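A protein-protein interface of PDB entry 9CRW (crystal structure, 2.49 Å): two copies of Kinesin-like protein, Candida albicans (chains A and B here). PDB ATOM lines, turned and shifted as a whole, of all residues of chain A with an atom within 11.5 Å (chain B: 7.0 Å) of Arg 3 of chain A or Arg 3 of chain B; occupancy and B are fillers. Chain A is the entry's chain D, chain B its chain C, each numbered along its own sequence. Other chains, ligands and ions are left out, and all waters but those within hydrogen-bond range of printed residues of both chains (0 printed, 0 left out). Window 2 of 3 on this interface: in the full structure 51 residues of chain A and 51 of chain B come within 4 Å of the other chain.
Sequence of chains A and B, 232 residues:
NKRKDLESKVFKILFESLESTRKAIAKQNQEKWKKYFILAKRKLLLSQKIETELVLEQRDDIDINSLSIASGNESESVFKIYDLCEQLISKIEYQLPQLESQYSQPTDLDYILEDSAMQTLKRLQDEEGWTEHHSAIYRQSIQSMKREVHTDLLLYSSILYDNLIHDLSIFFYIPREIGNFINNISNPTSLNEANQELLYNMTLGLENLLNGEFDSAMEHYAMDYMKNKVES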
ATOM      1  N   ASN A   1      21.860  29.639 -22.831  1.00  0.00           N
ATOM      2  CA  ASN A   1      20.559  29.267 -22.289  1.00  0.00           C
ATOM      3  C   ASN A   1      19.747  28.409 -23.263  1.00  0.00           C
ATOM      4  O   ASN A   1      18.520  28.336 -23.145  1.00  0.00           O
ATOM      5  CB  ASN A   1      19.759  30.519 -21.913  1.00  0.00           C
ATOM      6  CG  ASN A   1      20.395  31.295 -20.777  1.00  0.00           C
ATOM      7  OD1 ASN A   1      20.966  30.711 -19.852  1.00  0.00           O
ATOM      8  ND2 ASN A   1      20.301  32.619 -20.838  1.00  0.00           N
ATOM      9  N   LYS A   2      20.423  27.774 -24.226  1.00  0.00           N
ATOM     10  CA  LYS A   2      19.730  26.841 -25.109  1.00  0.00           C
ATOM     11  C   LYS A   2      19.136  25.685 -24.310  1.00  0.00           C
ATOM     12  O   LYS A   2      17.980  25.296 -24.531  1.00  0.00           O
ATOM     13  CB  LYS A   2      20.684  26.337 -26.196  1.00  0.00           C
ATOM     14  CG  LYS A   2      21.037  27.435 -27.193  1.00  0.00           C
ATOM     15  CD  LYS A   2      22.085  27.033 -28.226  1.00  0.00           C
ATOM     16  CE  LYS A   2      22.377  28.214 -29.157  1.00  0.00           C
ATOM     17  NZ  LYS A   2      23.400  27.924 -30.196  1.00  0.00           N
ATOM     18  N   ARG A   3      19.896  25.166 -23.337  1.00  0.00           N
ATOM     19  CA  ARG A   3      19.409  24.183 -22.380  1.00  0.00           C
ATOM     20  C   ARG A   3      18.561  24.796 -21.268  1.00  0.00           C
ATOM     21  O   ARG A   3      17.807  24.065 -20.620  1.00  0.00           O
ATOM     22  CB  ARG A   3      20.584  23.398 -21.781  1.00  0.00           C
ATOM     23  CG  ARG A   3      21.187  23.942 -20.488  1.00  0.00           C
ATOM     24  CD  ARG A   3      21.711  25.390 -20.572  1.00  0.00           C
ATOM     25  NE  ARG A   3      22.218  25.776 -21.883  1.00  0.00           N
ATOM     26  CZ  ARG A   3      23.388  25.410 -22.391  1.00  0.00           C
ATOM     27  NH1 ARG A   3      24.206  24.603 -21.736  1.00  0.00           N
ATOM     28  NH2 ARG A   3      23.743  25.861 -23.592  1.00  0.00           N
ATOM     29  N   LYS A   4      18.626  26.112 -21.050  1.00  0.00           N
ATOM     30  CA  LYS A   4      17.654  26.747 -20.162  1.00  0.00           C
ATOM     31  C   LYS A   4      16.261  26.713 -20.770  1.00  0.00           C
ATOM     32  O   LYS A   4      15.300  26.316 -20.110  1.00  0.00           O
ATOM     33  CB  LYS A   4      18.055  28.195 -19.847  1.00  0.00           C
ATOM     34  CG  LYS A   4      17.057  28.978 -18.945  1.00  0.00           C
ATOM     35  CD  LYS A   4      15.895  29.622 -19.719  1.00  0.00           C
ATOM     36  CE  LYS A   4      14.958  30.387 -18.807  1.00  0.00           C
ATOM     37  NZ  LYS A   4      15.487  31.752 -18.596  1.00  0.00           N
ATOM     38  N   ASP A   5      16.119  27.190 -22.006  1.00  0.00           N
ATOM     39  CA  ASP A   5      14.823  27.062 -22.660  1.00  0.00           C
ATOM     40  C   ASP A   5      14.459  25.602 -22.876  1.00  0.00           C
ATOM     41  O   ASP A   5      13.283  25.251 -22.771  1.00  0.00           O
ATOM     42  CB  ASP A   5      14.812  27.838 -23.975  1.00  0.00           C
ATOM     43  CG  ASP A   5      14.755  29.336 -23.752  1.00  0.00           C
ATOM     44  OD1 ASP A   5      13.843  29.789 -23.026  1.00  0.00           O
ATOM     45  OD2 ASP A   5      15.629  30.054 -24.286  1.00  0.00           O
ATOM     46  N   LEU A   6      15.445  24.733 -23.126  1.00  0.00           N
ATOM     47  CA  LEU A   6      15.194  23.294 -23.106  1.00  0.00           C
ATOM     48  C   LEU A   6      14.496  22.859 -21.819  1.00  0.00           C
ATOM     49  O   LEU A   6      13.358  22.391 -21.879  1.00  0.00           O
ATOM     50  CB  LEU A   6      16.487  22.501 -23.269  1.00  0.00           C
ATOM     51  CG  LEU A   6      16.319  20.993 -23.082  1.00  0.00           C
ATOM     52  CD1 LEU A   6      15.743  20.356 -24.339  1.00  0.00           C
ATOM     53  CD2 LEU A   6      17.631  20.329 -22.671  1.00  0.00           C
ATOM     54  N   GLU A   7      15.165  22.989 -20.664  1.00  0.00           N
ATOM     55  CA  GLU A   7      14.575  22.539 -19.404  1.00  0.00           C
ATOM     56  C   GLU A   7      13.260  23.261 -19.119  1.00  0.00           C
ATOM     57  O   GLU A   7      12.273  22.625 -18.733  1.00  0.00           O
ATOM     58  CB  GLU A   7      15.565  22.727 -18.244  1.00  0.00           C
ATOM     59  CG  GLU A   7      15.339  21.778 -17.035  1.00  0.00           C
ATOM     60  CD  GLU A   7      16.193  22.128 -15.795  1.00  0.00           C
ATOM     61  OE1 GLU A   7      16.320  23.330 -15.475  1.00  0.00           O
ATOM     62  OE2 GLU A   7      16.733  21.203 -15.131  1.00  0.00           O
ATOM     63  N   SER A   8      13.215  24.585 -19.335  1.00  0.00           N
ATOM     64  CA  SER A   8      12.017  25.374 -19.050  1.00  0.00           C
ATOM     65  C   SER A   8      10.818  24.890 -19.859  1.00  0.00           C
ATOM     66  O   SER A   8       9.717  24.720 -19.318  1.00  0.00           O
ATOM     67  CB  SER A   8      12.277  26.856 -19.332  1.00  0.00           C
ATOM     68  OG  SER A   8      12.736  27.544 -18.181  1.00  0.00           O
ATOM     69  N   LYS A   9      11.004  24.632 -21.150  1.00  0.00           N
ATOM     70  CA  LYS A   9       9.851  24.278 -21.960  1.00  0.00           C
ATOM     71  C   LYS A   9       9.565  22.782 -21.969  1.00  0.00           C
ATOM     72  O   LYS A   9       8.424  22.405 -22.237  1.00  0.00           O
ATOM     73  CB  LYS A   9      10.023  24.826 -23.378  1.00  0.00           C
ATOM     74  CG  LYS A   9      10.370  26.326 -23.391  1.00  0.00           C
ATOM     75  CD  LYS A   9       9.488  27.138 -22.441  1.00  0.00           C
ATOM     76  CE  LYS A   9      10.137  28.474 -22.085  1.00  0.00           C
ATOM     77  NZ  LYS A   9       9.249  29.332 -21.243  1.00  0.00           N
ATOM     78  N   VAL A  10      10.539  21.924 -21.627  1.00  0.00           N
ATOM     79  CA  VAL A  10      10.210  20.516 -21.374  1.00  0.00           C
ATOM     80  C   VAL A  10       9.453  20.389 -20.058  1.00  0.00           C
ATOM     81  O   VAL A  10       8.655  19.464 -19.878  1.00  0.00           O
ATOM     82  CB  VAL A  10      11.456  19.601 -21.396  1.00  0.00           C
ATOM     83  CG1 VAL A  10      12.442  19.986 -20.330  1.00  0.00           C
ATOM     84  CG2 VAL A  10      11.065  18.131 -21.185  1.00  0.00           C
ATOM     85  N   PHE A  11       9.682  21.301 -19.117  1.00  0.00           N
ATOM     86  CA  PHE A  11       8.762  21.410 -17.994  1.00  0.00           C
ATOM     87  C   PHE A  11       7.399  21.923 -18.471  1.00  0.00           C
ATOM     88  O   PHE A  11       6.350  21.409 -18.046  1.00  0.00           O
ATOM     89  CB  PHE A  11       9.354  22.311 -16.898  1.00  0.00           C
ATOM     90  CG  PHE A  11      10.284  21.598 -15.925  1.00  0.00           C
ATOM     91  CD1 PHE A  11      10.076  20.271 -15.570  1.00  0.00           C
ATOM     92  CD2 PHE A  11      11.367  22.261 -15.362  1.00  0.00           C
ATOM     93  CE1 PHE A  11      10.930  19.617 -14.671  1.00  0.00           C
ATOM     94  CE2 PHE A  11      12.221  21.615 -14.458  1.00  0.00           C
ATOM     95  CZ  PHE A  11      12.001  20.289 -14.118  1.00  0.00           C
ATOM     96  N   LYS A  12       7.404  22.933 -19.352  1.00  0.00           N
ATOM     97  CA  LYS A  12       6.164  23.552 -19.814  1.00  0.00           C
ATOM     98  C   LYS A  12       5.248  22.532 -20.488  1.00  0.00           C
ATOM     99  O   LYS A  12       4.035  22.504 -20.238  1.00  0.00           O
ATOM    100  CB  LYS A  12       6.489  24.698 -20.773  1.00  0.00           C
ATOM    101  CG  LYS A  12       5.291  25.528 -21.174  1.00  0.00           C
ATOM    102  CD  LYS A  12       4.680  26.182 -19.951  1.00  0.00           C
ATOM    103  CE  LYS A  12       3.161  26.147 -19.998  1.00  0.00           C
ATOM    104  NZ  LYS A  12       2.598  27.011 -21.076  1.00  0.00           N
ATOM    105  N   GLU A 128      12.966  16.018 -26.653  1.00  0.00           N
ATOM    106  CA  GLU A 128      14.342  16.431 -26.428  1.00  0.00           C
ATOM    107  C   GLU A 128      14.495  16.972 -25.007  1.00  0.00           C
ATOM    108  O   GLU A 128      13.738  17.851 -24.578  1.00  0.00           O
ATOM    109  CB  GLU A 128      14.727  17.482 -27.466  1.00  0.00           C
ATOM    110  CG  GLU A 128      16.211  17.763 -27.586  1.00  0.00           C
ATOM    111  CD  GLU A 128      16.470  18.949 -28.483  1.00  0.00           C
ATOM    112  OE1 GLU A 128      15.488  19.435 -29.093  1.00  0.00           O
ATOM    113  OE2 GLU A 128      17.636  19.397 -28.574  1.00  0.00           O
ATOM    114  N   GLY A 129      15.476  16.446 -24.273  1.00  0.00           N
ATOM    115  CA  GLY A 129      15.653  16.843 -22.893  1.00  0.00           C
ATOM    116  C   GLY A 129      14.680  16.207 -21.924  1.00  0.00           C
ATOM    117  O   GLY A 129      14.624  16.619 -20.759  1.00  0.00           O
ATOM    118  N   TRP A 130      13.905  15.224 -22.371  1.00  0.00           N
ATOM    119  CA  TRP A 130      13.019  14.479 -21.491  1.00  0.00           C
ATOM    120  C   TRP A 130      13.788  13.343 -20.816  1.00  0.00           C
ATOM    121  O   TRP A 130      14.648  12.710 -21.431  1.00  0.00           O
ATOM    122  CB  TRP A 130      11.841  13.934 -22.303  1.00  0.00           C
ATOM    123  CG  TRP A 130      10.854  13.121 -21.516  1.00  0.00           C
ATOM    124  CD1 TRP A 130      10.959  11.799 -21.184  1.00  0.00           C
ATOM    125  CD2 TRP A 130       9.606  13.574 -20.976  1.00  0.00           C
ATOM    126  NE1 TRP A 130       9.856  11.403 -20.461  1.00  0.00           N
ATOM    127  CE2 TRP A 130       9.009  12.474 -20.324  1.00  0.00           C
ATOM    128  CE3 TRP A 130       8.932  14.801 -20.983  1.00  0.00           C
ATOM    129  CZ2 TRP A 130       7.771  12.567 -19.686  1.00  0.00           C
ATOM    130  CZ3 TRP A 130       7.700  14.884 -20.350  1.00  0.00           C
ATOM    131  CH2 TRP A 130       7.130  13.777 -19.715  1.00  0.00           C
ATOM    132  N   THR A 131      13.483  13.088 -19.545  1.00  0.00           N
ATOM    133  CA  THR A 131      14.185  12.047 -18.808  1.00  0.00           C
ATOM    134  C   THR A 131      13.209  11.318 -17.900  1.00  0.00           C
ATOM    135  O   THR A 131      12.108  11.801 -17.621  1.00  0.00           O
ATOM    136  CB  THR A 131      15.356  12.609 -17.987  1.00  0.00           C
ATOM    137  OG1 THR A 131      16.000  11.534 -17.295  1.00  0.00           O
ATOM    138  CG2 THR A 131      14.874  13.643 -16.985  1.00  0.00           C
ATOM    139  N   GLU A 132      13.627  10.134 -17.445  1.00  0.00           N
ATOM    140  CA  GLU A 132      12.723   9.273 -16.689  1.00  0.00           C
ATOM    141  C   GLU A 132      12.243   9.933 -15.401  1.00  0.00           C
ATOM    142  O   GLU A 132      11.220   9.508 -14.849  1.00  0.00           O
ATOM    143  CB  GLU A 132      13.391   7.924 -16.400  1.00  0.00           C
ATOM    144  CG  GLU A 132      14.239   7.876 -15.128  1.00  0.00           C
ATOM    145  CD  GLU A 132      15.678   8.363 -15.326  1.00  0.00           C
ATOM    146  OE1 GLU A 132      16.151   8.391 -16.490  1.00  0.00           O
ATOM    147  OE2 GLU A 132      16.334   8.712 -14.309  1.00  0.00           O
ATOM    148  N   HIS A 133      12.939  10.970 -14.918  1.00  0.00           N
ATOM    149  CA  HIS A 133      12.402  11.767 -13.817  1.00  0.00           C
ATOM    150  C   HIS A 133      11.144  12.513 -14.239  1.00  0.00           C
ATOM    151  O   HIS A 133      10.161  12.577 -13.480  1.00  0.00           O
ATOM    152  CB  HIS A 133      13.450  12.763 -13.323  1.00  0.00           C
ATOM    153  CG  HIS A 133      14.554  12.128 -12.542  1.00  0.00           C
ATOM    154  ND1 HIS A 133      14.350  11.032 -11.730  1.00  0.00           N
ATOM    155  CD2 HIS A 133      15.872  12.426 -12.455  1.00  0.00           C
ATOM    156  CE1 HIS A 133      15.498  10.687 -11.172  1.00  0.00           C
ATOM    157  NE2 HIS A 133      16.436  11.519 -11.592  1.00  0.00           N
ATOM    158  N   HIS A 134      11.169  13.106 -15.440  1.00  0.00           N
ATOM    159  CA  HIS A 134       9.957  13.695 -15.995  1.00  0.00           C
ATOM    160  C   HIS A 134       8.832  12.660 -16.037  1.00  0.00           C
ATOM    161  O   HIS A 134       7.698  12.946 -15.627  1.00  0.00           O
ATOM    162  CB  HIS A 134      10.242  14.280 -17.385  1.00  0.00           C
ATOM    163  CG  HIS A 134      11.080  15.533 -17.373  1.00  0.00           C
ATOM    164  ND1 HIS A 134      12.459  15.512 -17.419  1.00  0.00           N
ATOM    165  CD2 HIS A 134      10.728  16.844 -17.339  1.00  0.00           C
ATOM    166  CE1 HIS A 134      12.920  16.752 -17.404  1.00  0.00           C
ATOM    167  NE2 HIS A 134      11.891  17.581 -17.359  1.00  0.00           N
ATOM    168  N   LYS B   2      27.280  16.052 -15.550  1.00  0.00           N
ATOM    169  CA  LYS B   2      27.330  17.387 -16.139  1.00  0.00           C
ATOM    170  C   LYS B   2      26.166  18.228 -15.595  1.00  0.00           C
ATOM    171  O   LYS B   2      25.903  18.199 -14.394  1.00  0.00           O
ATOM    172  CB  LYS B   2      27.294  17.284 -17.661  1.00  0.00           C
ATOM    173  CG  LYS B   2      28.090  16.091 -18.204  1.00  0.00           C
ATOM    174  CD  LYS B   2      29.547  16.069 -17.710  1.00  0.00           C
ATOM    175  CE  LYS B   2      30.384  17.194 -18.308  1.00  0.00           C
ATOM    176  NZ  LYS B   2      30.414  17.159 -19.800  1.00  0.00           N
ATOM    177  N   ARG B   3      25.470  18.989 -16.446  1.00  0.00           N
ATOM    178  CA  ARG B   3      24.172  19.505 -16.017  1.00  0.00           C
ATOM    179  C   ARG B   3      23.150  18.379 -15.900  1.00  0.00           C
ATOM    180  O   ARG B   3      22.153  18.522 -15.183  1.00  0.00           O
ATOM    181  CB  ARG B   3      23.668  20.600 -16.964  1.00  0.00           C
ATOM    182  CG  ARG B   3      22.218  20.996 -16.717  1.00  0.00           C
ATOM    183  CD  ARG B   3      21.924  22.423 -17.061  1.00  0.00           C
ATOM    184  NE  ARG B   3      20.752  22.872 -16.325  1.00  0.00           N
ATOM    185  CZ  ARG B   3      20.213  24.081 -16.418  1.00  0.00           C
ATOM    186  NH1 ARG B   3      20.685  24.986 -17.264  1.00  0.00           N
ATOM    187  NH2 ARG B   3      19.178  24.390 -15.635  1.00  0.00           N
ATOM    188  N   LYS B   4      23.398  17.250 -16.573  1.00  0.00           N
ATOM    189  CA  LYS B   4      22.576  16.061 -16.373  1.00  0.00           C
ATOM    190  C   LYS B   4      22.607  15.620 -14.914  1.00  0.00           C
ATOM    191  O   LYS B   4      21.559  15.332 -14.316  1.00  0.00           O
ATOM    192  CB  LYS B   4      23.054  14.939 -17.299  1.00  0.00           C
ATOM    193  CG  LYS B   4      22.197  13.671 -17.282  1.00  0.00           C
ATOM    194  CD  LYS B   4      22.687  12.649 -16.257  1.00  0.00           C
ATOM    195  CE  LYS B   4      24.125  12.233 -16.523  1.00  0.00           C
ATOM    196  NZ  LYS B   4      24.313  11.698 -17.899  1.00  0.00           N
ATOM    197  N   ASP B   5      23.805  15.557 -14.316  1.00  0.00           N
ATOM    198  CA  ASP B   5      23.879  15.165 -12.909  1.00  0.00           C
ATOM    199  C   ASP B   5      23.312  16.249 -11.998  1.00  0.00           C
ATOM    200  O   ASP B   5      22.821  15.936 -10.912  1.00  0.00           O
ATOM    201  CB  ASP B   5      25.319  14.783 -12.511  1.00  0.00           C
ATOM    202  CG  ASP B   5      26.257  15.983 -12.365  1.00  0.00           C
ATOM    203  OD1 ASP B   5      27.226  16.079 -13.153  1.00  0.00           O
ATOM    204  OD2 ASP B   5      26.047  16.812 -11.452  1.00  0.00           O
ATOM    205  N   LEU B   6      23.335  17.515 -12.433  1.00  0.00           N
ATOM    206  CA  LEU B   6      22.630  18.575 -11.708  1.00  0.00           C
ATOM    207  C   LEU B   6      21.130  18.305 -11.679  1.00  0.00           C
ATOM    208  O   LEU B   6      20.473  18.444 -10.641  1.00  0.00           O
ATOM    209  CB  LEU B   6      22.904  19.931 -12.365  1.00  0.00           C
ATOM    210  CG  LEU B   6      22.485  21.241 -11.677  1.00  0.00           C
ATOM    211  CD1 LEU B   6      20.955  21.487 -11.592  1.00  0.00           C
ATOM    212  CD2 LEU B   6      23.128  21.281 -10.312  1.00  0.00           C
ATOM    213  N   GLU B   7      20.569  17.966 -12.839  1.00  0.00           N
ATOM    214  CA  GLU B   7      19.150  17.658 -12.933  1.00  0.00           C
ATOM    215  C   GLU B   7      18.795  16.455 -12.073  1.00  0.00           C
ATOM    216  O   GLU B   7      17.761  16.451 -11.398  1.00  0.00           O
ATOM    217  CB  GLU B   7      18.769  17.407 -14.380  1.00  0.00           C
ATOM    218  CG  GLU B   7      17.877  18.446 -14.985  1.00  0.00           C
ATOM    219  CD  GLU B   7      17.599  18.129 -16.431  1.00  0.00           C
ATOM    220  OE1 GLU B   7      18.117  17.095 -16.900  1.00  0.00           O
ATOM    221  OE2 GLU B   7      16.876  18.896 -17.100  1.00  0.00           O
ATOM    222  N   SER B   8      19.640  15.418 -12.086  1.00  0.00           N
ATOM    223  CA  SER B   8      19.386  14.252 -11.240  1.00  0.00           C
ATOM    224  C   SER B   8      19.522  14.600  -9.761  1.00  0.00           C
ATOM    225  O   SER B   8      18.773  14.080  -8.928  1.00  0.00           O
ATOM    226  CB  SER B   8      20.327  13.106 -11.596  1.00  0.00           C
ATOM    227  OG  SER B   8      20.122  12.683 -12.921  1.00  0.00           O
ATOM    228  N   LYS B   9      20.465  15.481  -9.418  1.00  0.00           N
ATOM    229  CA  LYS B   9      20.620  15.926  -8.037  1.00  0.00           C
ATOM    230  C   LYS B   9      19.367  16.650  -7.557  1.00  0.00           C
ATOM    231  O   LYS B   9      18.822  16.337  -6.490  1.00  0.00           O
ATOM    232  CB  LYS B   9      21.856  16.829  -7.916  1.00  0.00           C
ATOM    233  CG  LYS B   9      21.995  17.588  -6.587  1.00  0.00           C
ATOM    234  CD  LYS B   9      22.994  18.740  -6.706  1.00  0.00           C
ATOM    235  CE  LYS B   9      22.983  19.650  -5.474  1.00  0.00           C
ATOM    236  NZ  LYS B   9      21.814  20.585  -5.432  1.00  0.00           N
ATOM    237  N   GLY B 129      20.477  24.005  -8.456  1.00  0.00           N
ATOM    238  CA  GLY B 129      19.681  24.194  -9.654  1.00  0.00           C
ATOM    239  C   GLY B 129      18.202  23.989  -9.404  1.00  0.00           C
ATOM    240  O   GLY B 129      17.566  23.162 -10.062  1.00  0.00           O
ATOM    241  N   THR B 131      14.693  25.522  -9.726  1.00  0.00           N
ATOM    242  CA  THR B 131      13.948  26.506 -10.488  1.00  0.00           C
ATOM    243  C   THR B 131      12.520  26.575  -9.975  1.00  0.00           C
ATOM    244  O   THR B 131      12.064  25.718  -9.216  1.00  0.00           O
ATOM    245  CB  THR B 131      13.960  26.131 -11.966  1.00  0.00           C
ATOM    246  OG1 THR B 131      12.996  25.093 -12.184  1.00  0.00           O
ATOM    247  CG2 THR B 131      15.337  25.600 -12.344  1.00  0.00           C
ATOM    248  N   HIS B 134      10.498  23.272 -10.362  1.00  0.00           N
ATOM    249  CA  HIS B 134      10.641  22.373  -9.215  1.00  0.00           C
ATOM    250  C   HIS B 134       9.740  22.815  -8.067  1.00  0.00           C
ATOM    251  O   HIS B 134       9.098  21.987  -7.403  1.00  0.00           O
ATOM    252  CB  HIS B 134      12.095  22.331  -8.753  1.00  0.00           C
ATOM    253  CG  HIS B 134      13.042  21.777  -9.770  1.00  0.00           C
ATOM    254  ND1 HIS B 134      13.642  22.559 -10.734  1.00  0.00           N
ATOM    255  CD2 HIS B 134      13.500  20.518  -9.967  1.00  0.00           C
ATOM    256  CE1 HIS B 134      14.422  21.802 -11.487  1.00  0.00           C
ATOM    257  NE2 HIS B 134      14.352  20.560 -11.042  1.00  0.00           N
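OE1 of Glu 7 of chain A is in salt-bridge range of NH2 of Arg 3 of chain B. OE2 of Glu 7 of chain A lies close to OE2 of Glu 7 of chain B.
OG1 of Thr 131 of chain B is in hydrogen-bond range of ND1 of His 134 of chain B, 3.0 Å away.
Among the printed residues, pairs that only touch across the chains: Arg 3 of chain A with Arg 3 of chain B, Glu 7 of chain A with Thr 131 of chain B and Phe 11 of chain A with His 134 of chain B.
Of chain B, only Arg 3 (3.4 Å) comes within 4 Å of Arg 3 of chain A. Asp 5 of chain A touches none of the printed residues of chain B. Of the printed residues of chain B, Phe 11 of chain A touches His 134 (3.7 Å). Of chain A, only Arg 3 and Glu 7 come within 4 Å of Arg 3 of chain B. No residue of chain A comes within 4 Å of Asp 5 of chain B. No residue of chain A comes within 4 Å of Leu 6 of chain B. Glu 7 of chain B touches just one residue of chain A: Glu 7 (3.0 Å). Gly 129 of chain B touches none of the printed residues of chain A. Of the printed residues of chain A, Thr 131 of chain B touches Glu 7 (3.99 Å).
Hydrophobic or aromatic side chains of chain B within 4 Å of the printed part of chain A: His 134. Among the printed residues, 5 pairs touch across the chains. Among the printed residues, Asp or Glu carboxylates within 4 Å of a Lys or Arg side-chain nitrogen of the other chain: Glu 7 of chain A with Arg 3 of chain B (3.1 Å).
Arg 3 of chain A touches its own counterpart, Arg 3 of chain B. Glu 7 of chain A touches Arg 3 of chain B, but with the chains exchanged Arg 3 of chain A does not touch Glu 7 of chain B (6.3 Å). Glu 7 of chain A touches its own counterpart, Glu 7 of chain B. Glu 7 of chain A touches Thr 131 of chain B, but with the chains exchanged Thr 131 of chain A does not touch Glu 7 of chain B (4.7 Å). 11 positions are printed for both chains. Of the 5 pairs that touch across the chains among the printed residues, 2 have their exchanged pair printed and touching as well.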
